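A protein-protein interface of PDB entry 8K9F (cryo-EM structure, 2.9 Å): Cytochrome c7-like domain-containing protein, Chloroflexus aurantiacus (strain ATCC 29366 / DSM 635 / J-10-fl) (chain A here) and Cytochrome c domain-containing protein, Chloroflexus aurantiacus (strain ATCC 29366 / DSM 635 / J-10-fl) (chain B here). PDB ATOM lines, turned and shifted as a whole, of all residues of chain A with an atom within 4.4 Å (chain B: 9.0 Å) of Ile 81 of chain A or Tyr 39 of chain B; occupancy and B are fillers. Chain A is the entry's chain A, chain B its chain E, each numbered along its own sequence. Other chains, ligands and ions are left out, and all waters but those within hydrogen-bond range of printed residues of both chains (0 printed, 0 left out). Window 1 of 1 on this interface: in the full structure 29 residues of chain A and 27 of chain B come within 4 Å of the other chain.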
ATOM      1  N   PHE A  78     -21.671   4.227  30.387  1.00  0.00           N
ATOM      2  CA  PHE A  78     -23.075   4.257  30.028  1.00  0.00           C
ATOM      3  C   PHE A  78     -23.298   3.283  28.893  1.00  0.00           C
ATOM      4  O   PHE A  78     -22.779   3.485  27.796  1.00  0.00           O
ATOM      5  CB  PHE A  78     -23.476   5.668  29.599  1.00  0.00           C
ATOM      6  CG  PHE A  78     -24.914   5.804  29.206  1.00  0.00           C
ATOM      7  CD1 PHE A  78     -25.902   5.808  30.164  1.00  0.00           C
ATOM      8  CD2 PHE A  78     -25.274   5.944  27.880  1.00  0.00           C
ATOM      9  CE1 PHE A  78     -27.226   5.943  29.819  1.00  0.00           C
ATOM     10  CE2 PHE A  78     -26.599   6.088  27.526  1.00  0.00           C
ATOM     11  CZ  PHE A  78     -27.575   6.081  28.499  1.00  0.00           C
ATOM     12  N   ALA A  79     -24.044   2.224  29.151  1.00  0.00           N
ATOM     13  CA  ALA A  79     -24.461   1.361  28.063  1.00  0.00           C
ATOM     14  C   ALA A  79     -25.516   2.122  27.276  1.00  0.00           C
ATOM     15  O   ALA A  79     -26.452   2.657  27.876  1.00  0.00           O
ATOM     16  CB  ALA A  79     -24.994   0.044  28.607  1.00  0.00           C
ATOM     17  N   ASN A  80     -25.349   2.203  25.951  1.00  0.00           N
ATOM     18  CA  ASN A  80     -26.116   3.144  25.136  1.00  0.00           C
ATOM     19  C   ASN A  80     -27.586   2.785  25.150  1.00  0.00           C
ATOM     20  O   ASN A  80     -27.953   1.629  24.944  1.00  0.00           O
ATOM     21  CB  ASN A  80     -25.615   3.162  23.693  1.00  0.00           C
ATOM     22  CG  ASN A  80     -26.561   3.887  22.762  1.00  0.00           C
ATOM     23  OD1 ASN A  80     -26.817   5.077  22.918  1.00  0.00           O
ATOM     24  ND2 ASN A  80     -27.104   3.162  21.791  1.00  0.00           N
ATOM     25  N   ILE A  81     -28.425   3.749  25.462  1.00  0.00           N
ATOM     26  CA  ILE A  81     -29.852   3.484  25.317  1.00  0.00           C
ATOM     27  C   ILE A  81     -30.228   3.648  23.848  1.00  0.00           C
ATOM     28  O   ILE A  81     -29.786   4.620  23.206  1.00  0.00           O
ATOM     29  CB  ILE A  81     -30.654   4.393  26.247  1.00  0.00           C
ATOM     30  CG1 ILE A  81     -30.800   3.715  27.612  1.00  0.00           C
ATOM     31  CG2 ILE A  81     -32.027   4.670  25.729  1.00  0.00           C
ATOM     32  CD1 ILE A  81     -31.595   2.413  27.596  1.00  0.00           C
ATOM     33  N   PRO A  82     -30.932   2.681  23.262  1.00  0.00           N
ATOM     34  CA  PRO A  82     -31.123   2.659  21.808  1.00  0.00           C
ATOM     35  C   PRO A  82     -31.945   3.831  21.301  1.00  0.00           C
ATOM     36  O   PRO A  82     -32.978   4.190  21.869  1.00  0.00           O
ATOM     37  CB  PRO A  82     -31.851   1.330  21.568  1.00  0.00           C
ATOM     38  CG  PRO A  82     -31.671   0.564  22.808  1.00  0.00           C
ATOM     39  CD  PRO A  82     -31.520   1.508  23.916  1.00  0.00           C
ATOM     40  N   ALA A  83     -31.460   4.426  20.216  1.00  0.00           N
ATOM     41  CA  ALA A  83     -32.124   5.544  19.572  1.00  0.00           C
ATOM     42  C   ALA A  83     -33.321   5.054  18.763  1.00  0.00           C
ATOM     43  O   ALA A  83     -33.636   3.862  18.715  1.00  0.00           O
ATOM     44  CB  ALA A  83     -31.136   6.287  18.682  1.00  0.00           C
ATOM     45  N   TRP A 116     -38.335   6.770  27.485  1.00  0.00           N
ATOM     46  CA  TRP A 116     -38.259   5.503  28.202  1.00  0.00           C
ATOM     47  C   TRP A 116     -38.135   5.739  29.700  1.00  0.00           C
ATOM     48  O   TRP A 116     -37.730   6.810  30.158  1.00  0.00           O
ATOM     49  CB  TRP A 116     -37.070   4.652  27.742  1.00  0.00           C
ATOM     50  CG  TRP A 116     -36.997   4.352  26.275  1.00  0.00           C
ATOM     51  CD1 TRP A 116     -36.177   4.939  25.368  1.00  0.00           C
ATOM     52  CD2 TRP A 116     -37.748   3.366  25.558  1.00  0.00           C
ATOM     53  NE1 TRP A 116     -36.377   4.398  24.127  1.00  0.00           N
ATOM     54  CE2 TRP A 116     -37.336   3.424  24.219  1.00  0.00           C
ATOM     55  CE3 TRP A 116     -38.728   2.440  25.921  1.00  0.00           C
ATOM     56  CZ2 TRP A 116     -37.890   2.618  23.238  1.00  0.00           C
ATOM     57  CZ3 TRP A 116     -39.256   1.623  24.953  1.00  0.00           C
ATOM     58  CH2 TRP A 116     -38.826   1.707  23.631  1.00  0.00           C
ATOM     59  N   LYS B  35     -27.230  18.295  38.001  1.00  0.00           N
ATOM     60  CA  LYS B  35     -26.471  18.180  36.767  1.00  0.00           C
ATOM     61  C   LYS B  35     -27.198  17.294  35.762  1.00  0.00           C
ATOM     62  O   LYS B  35     -28.104  16.531  36.103  1.00  0.00           O
ATOM     63  CB  LYS B  35     -25.088  17.604  37.046  1.00  0.00           C
ATOM     64  CG  LYS B  35     -25.120  16.181  37.551  1.00  0.00           C
ATOM     65  CD  LYS B  35     -23.796  15.783  38.144  1.00  0.00           C
ATOM     66  CE  LYS B  35     -23.662  14.291  38.198  1.00  0.00           C
ATOM     67  NZ  LYS B  35     -22.430  13.894  38.907  1.00  0.00           N
ATOM     68  N   TYR B  36     -26.793  17.413  34.504  1.00  0.00           N
ATOM     69  CA  TYR B  36     -27.358  16.594  33.444  1.00  0.00           C
ATOM     70  C   TYR B  36     -26.461  15.397  33.184  1.00  0.00           C
ATOM     71  O   TYR B  36     -25.257  15.548  32.963  1.00  0.00           O
ATOM     72  CB  TYR B  36     -27.549  17.416  32.171  1.00  0.00           C
ATOM     73  CG  TYR B  36     -28.740  18.324  32.268  1.00  0.00           C
ATOM     74  CD1 TYR B  36     -30.011  17.856  31.987  1.00  0.00           C
ATOM     75  CD2 TYR B  36     -28.601  19.635  32.684  1.00  0.00           C
ATOM     76  CE1 TYR B  36     -31.107  18.675  32.092  1.00  0.00           C
ATOM     77  CE2 TYR B  36     -29.692  20.463  32.791  1.00  0.00           C
ATOM     78  CZ  TYR B  36     -30.941  19.976  32.495  1.00  0.00           C
ATOM     79  OH  TYR B  36     -32.031  20.802  32.604  1.00  0.00           O
ATOM     80  N   THR B  37     -27.061  14.209  33.203  1.00  0.00           N
ATOM     81  CA  THR B  37     -26.355  12.951  32.999  1.00  0.00           C
ATOM     82  C   THR B  37     -26.288  12.704  31.492  1.00  0.00           C
ATOM     83  O   THR B  37     -26.483  13.646  30.716  1.00  0.00           O
ATOM     84  CB  THR B  37     -27.067  11.837  33.769  1.00  0.00           C
ATOM     85  OG1 THR B  37     -27.611  12.396  34.967  1.00  0.00           O
ATOM     86  CG2 THR B  37     -26.077  10.757  34.231  1.00  0.00           C
ATOM     87  N   THR B  38     -25.975  11.476  31.060  1.00  0.00           N
ATOM     88  CA  THR B  38     -25.769  11.208  29.639  1.00  0.00           C
ATOM     89  C   THR B  38     -27.049  11.410  28.837  1.00  0.00           C
ATOM     90  O   THR B  38     -27.074  12.200  27.888  1.00  0.00           O
ATOM     91  CB  THR B  38     -25.241   9.792  29.440  1.00  0.00           C
ATOM     92  OG1 THR B  38     -23.941   9.684  30.027  1.00  0.00           O
ATOM     93  CG2 THR B  38     -25.126   9.498  27.960  1.00  0.00           C
ATOM     94  N   TYR B  39     -28.138  10.759  29.241  1.00  0.00           N
ATOM     95  CA  TYR B  39     -29.417  10.911  28.561  1.00  0.00           C
ATOM     96  C   TYR B  39     -30.483  11.447  29.509  1.00  0.00           C
ATOM     97  O   TYR B  39     -31.646  11.048  29.432  1.00  0.00           O
ATOM     98  CB  TYR B  39     -29.879   9.591  27.947  1.00  0.00           C
ATOM     99  CG  TYR B  39     -29.196   9.201  26.657  1.00  0.00           C
ATOM    100  CD1 TYR B  39     -28.423  10.104  25.958  1.00  0.00           C
ATOM    101  CD2 TYR B  39     -29.343   7.920  26.133  1.00  0.00           C
ATOM    102  CE1 TYR B  39     -27.799   9.750  24.794  1.00  0.00           C
ATOM    103  CE2 TYR B  39     -28.718   7.553  24.961  1.00  0.00           C
ATOM    104  CZ  TYR B  39     -27.950   8.477  24.297  1.00  0.00           C
ATOM    105  OH  TYR B  39     -27.323   8.137  23.127  1.00  0.00           O
ATOM    106  N   GLU B  40     -30.092  12.322  30.429  1.00  0.00           N
ATOM    107  CA  GLU B  40     -31.060  13.012  31.266  1.00  0.00           C
ATOM    108  C   GLU B  40     -31.906  13.941  30.396  1.00  0.00           C
ATOM    109  O   GLU B  40     -31.377  14.590  29.496  1.00  0.00           O
ATOM    110  CB  GLU B  40     -30.342  13.809  32.357  1.00  0.00           C
ATOM    111  CG  GLU B  40     -31.243  14.390  33.446  1.00  0.00           C
ATOM    112  CD  GLU B  40     -30.564  14.449  34.807  1.00  0.00           C
ATOM    113  OE1 GLU B  40     -29.910  13.459  35.193  1.00  0.00           O
ATOM    114  OE2 GLU B  40     -30.695  15.480  35.501  1.00  0.00           O
ATOM    115  N   PRO B  41     -33.220  13.977  30.590  1.00  0.00           N
ATOM    116  CA  PRO B  41     -34.050  14.875  29.784  1.00  0.00           C
ATOM    117  C   PRO B  41     -33.894  16.317  30.225  1.00  0.00           C
ATOM    118  O   PRO B  41     -33.703  16.615  31.406  1.00  0.00           O
ATOM    119  CB  PRO B  41     -35.476  14.373  30.037  1.00  0.00           C
ATOM    120  CG  PRO B  41     -35.318  13.050  30.677  1.00  0.00           C
ATOM    121  CD  PRO B  41     -34.036  13.089  31.422  1.00  0.00           C
ATOM    122  N   SER B  42     -33.986  17.223  29.254  1.00  0.00           N
ATOM    123  CA  SER B  42     -33.812  18.646  29.497  1.00  0.00           C
ATOM    124  C   SER B  42     -35.026  19.410  28.999  1.00  0.00           C
ATOM    125  O   SER B  42     -35.465  19.214  27.863  1.00  0.00           O
ATOM    126  CB  SER B  42     -32.560  19.176  28.807  1.00  0.00           C
ATOM    127  OG  SER B  42     -32.523  20.591  28.875  1.00  0.00           O
ATOM    128  N   GLY B  48     -36.151  18.061  23.802  1.00  0.00           N
ATOM    129  CA  GLY B  48     -36.255  17.302  25.024  1.00  0.00           C
ATOM    130  C   GLY B  48     -35.078  16.400  25.291  1.00  0.00           C
ATOM    131  O   GLY B  48     -35.254  15.353  25.919  1.00  0.00           O
ATOM    132  N   ARG B  49     -33.892  16.766  24.823  1.00  0.00           N
ATOM    133  CA  ARG B  49     -32.681  15.981  24.981  1.00  0.00           C
ATOM    134  C   ARG B  49     -31.584  16.889  25.500  1.00  0.00           C
ATOM    135  O   ARG B  49     -31.323  17.936  24.903  1.00  0.00           O
ATOM    136  CB  ARG B  49     -32.250  15.384  23.648  1.00  0.00           C
ATOM    137  CG  ARG B  49     -32.340  13.898  23.539  1.00  0.00           C
ATOM    138  CD  ARG B  49     -31.749  13.497  22.219  1.00  0.00           C
ATOM    139  NE  ARG B  49     -32.241  14.341  21.141  1.00  0.00           N
ATOM    140  CZ  ARG B  49     -33.263  14.032  20.355  1.00  0.00           C
ATOM    141  NH1 ARG B  49     -33.911  12.889  20.484  1.00  0.00           N
ATOM    142  NH2 ARG B  49     -33.642  14.892  19.417  1.00  0.00           N
ATOM    143  N   SER B  50     -30.939  16.498  26.597  1.00  0.00           N
ATOM    144  CA  SER B  50     -29.771  17.248  27.044  1.00  0.00           C
ATOM    145  C   SER B  50     -28.576  16.975  26.150  1.00  0.00           C
ATOM    146  O   SER B  50     -27.760  17.867  25.900  1.00  0.00           O
ATOM    147  CB  SER B  50     -29.425  16.909  28.487  1.00  0.00           C
ATOM    148  OG  SER B  50     -28.266  17.606  28.896  1.00  0.00           O
ATOM    149  N   SER B  51     -28.452  15.743  25.670  1.00  0.00           N
ATOM    150  CA  SER B  51     -27.339  15.368  24.816  1.00  0.00           C
ATOM    151  C   SER B  51     -27.552  15.960  23.434  1.00  0.00           C
ATOM    152  O   SER B  51     -28.551  15.668  22.771  1.00  0.00           O
ATOM    153  CB  SER B  51     -27.229  13.850  24.747  1.00  0.00           C
ATOM    154  OG  SER B  51     -28.378  13.292  24.137  1.00  0.00           O
ATOM    155  N   ARG B  52     -26.670  16.747  23.025  1.00  0.00           N
ATOM    156  CA  ARG B  52     -26.924  17.504  21.819  1.00  0.00           C
ATOM    157  C   ARG B  52     -26.359  16.790  20.599  1.00  0.00           C
ATOM    158  O   ARG B  52     -25.386  16.040  20.712  1.00  0.00           O
ATOM    159  CB  ARG B  52     -26.314  18.901  21.953  1.00  0.00           C
ATOM    160  CG  ARG B  52     -27.037  19.771  22.961  1.00  0.00           C
ATOM    161  CD  ARG B  52     -28.293  20.357  22.356  1.00  0.00           C
ATOM    162  NE  ARG B  52     -29.478  19.547  22.601  1.00  0.00           N
ATOM    163  CZ  ARG B  52     -30.548  19.548  21.818  1.00  0.00           C
ATOM    164  NH1 ARG B  52     -30.610  20.304  20.738  1.00  0.00           N
ATOM    165  NH2 ARG B  52     -31.578  18.767  22.126  1.00  0.00           N
ATOM    166  N   ARG B 168     -23.397   3.612  14.458  1.00  0.00           N
ATOM    167  CA  ARG B 168     -23.121   2.534  15.395  1.00  0.00           C
ATOM    168  C   ARG B 168     -21.739   1.924  15.227  1.00  0.00           C
ATOM    169  O   ARG B 168     -21.154   1.466  16.213  1.00  0.00           O
ATOM    170  CB  ARG B 168     -24.179   1.439  15.268  1.00  0.00           C
ATOM    171  CG  ARG B 168     -25.375   1.658  16.165  1.00  0.00           C
ATOM    172  CD  ARG B 168     -26.589   0.912  15.681  1.00  0.00           C
ATOM    173  NE  ARG B 168     -27.083   1.461  14.428  1.00  0.00           N
ATOM    174  CZ  ARG B 168     -28.202   1.073  13.836  1.00  0.00           C
ATOM    175  NH1 ARG B 168     -28.973   0.140  14.367  1.00  0.00           N
ATOM    176  NH2 ARG B 168     -28.551   1.631  12.681  1.00  0.00           N
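The side-chain hydroxyl (OH) of Tyr 39 of chain B is in hydrogen-bond range of the side-chain amide oxygen (OD1) of Asn 80 of chain A.
Thr 38 of chain B touches Phe 78 of chain A.
CZ of Phe 78 of chain A touches CD2 of Tyr 39 of chain B (3.5 Å).
CE2 of Tyr 39 of chain B touches O of Ile 81 of chain A, at 3.6 Å.
Of chain B, only Tyr 39 comes within 4 Å of Ile 81 of chain A.
Tyr 39 of chain B touches just these residues of chain A: Phe 78, Asn 80 and Ile 81.
Of the printed residues of chain B, Phe 78 of chain A touches Thr 38 (3.6 Å) and Tyr 39 (3.5 Å).
Printed residues of chain A within 4 Å of Thr 38 of chain B: Phe 78.
Arg 49 of chain B touches none of the printed residues of chain A.
The nearest residue of chain B that does not touch Ile 81 of chain A is Thr 38 of chain B (7.1 Å).
The nearest printed residue of chain A that does not touch Tyr 39 of chain B is Pro 82 of chain A (5.6 Å).
Of the 7 printed residues of chain A, 3 touch a printed residue of chain B.
Printed residues of chain A that touch a printed residue of chain B: Phe 78, Asn 80 and Ile 81.
Hydrophobic or aromatic side chains of chain A that line the printed part of chain B: Phe 78 and Ile 81.
Of the 14 printed residues of chain B, 2 touch a printed residue of chain A.
Hydrophobic or aromatic side chains of chain B that line the printed part of chain A: Tyr 39.
Among the printed residues, no Asp or Glu carboxylate lies within 4 Å of a Lys or Arg side-chain nitrogen of the other chain.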
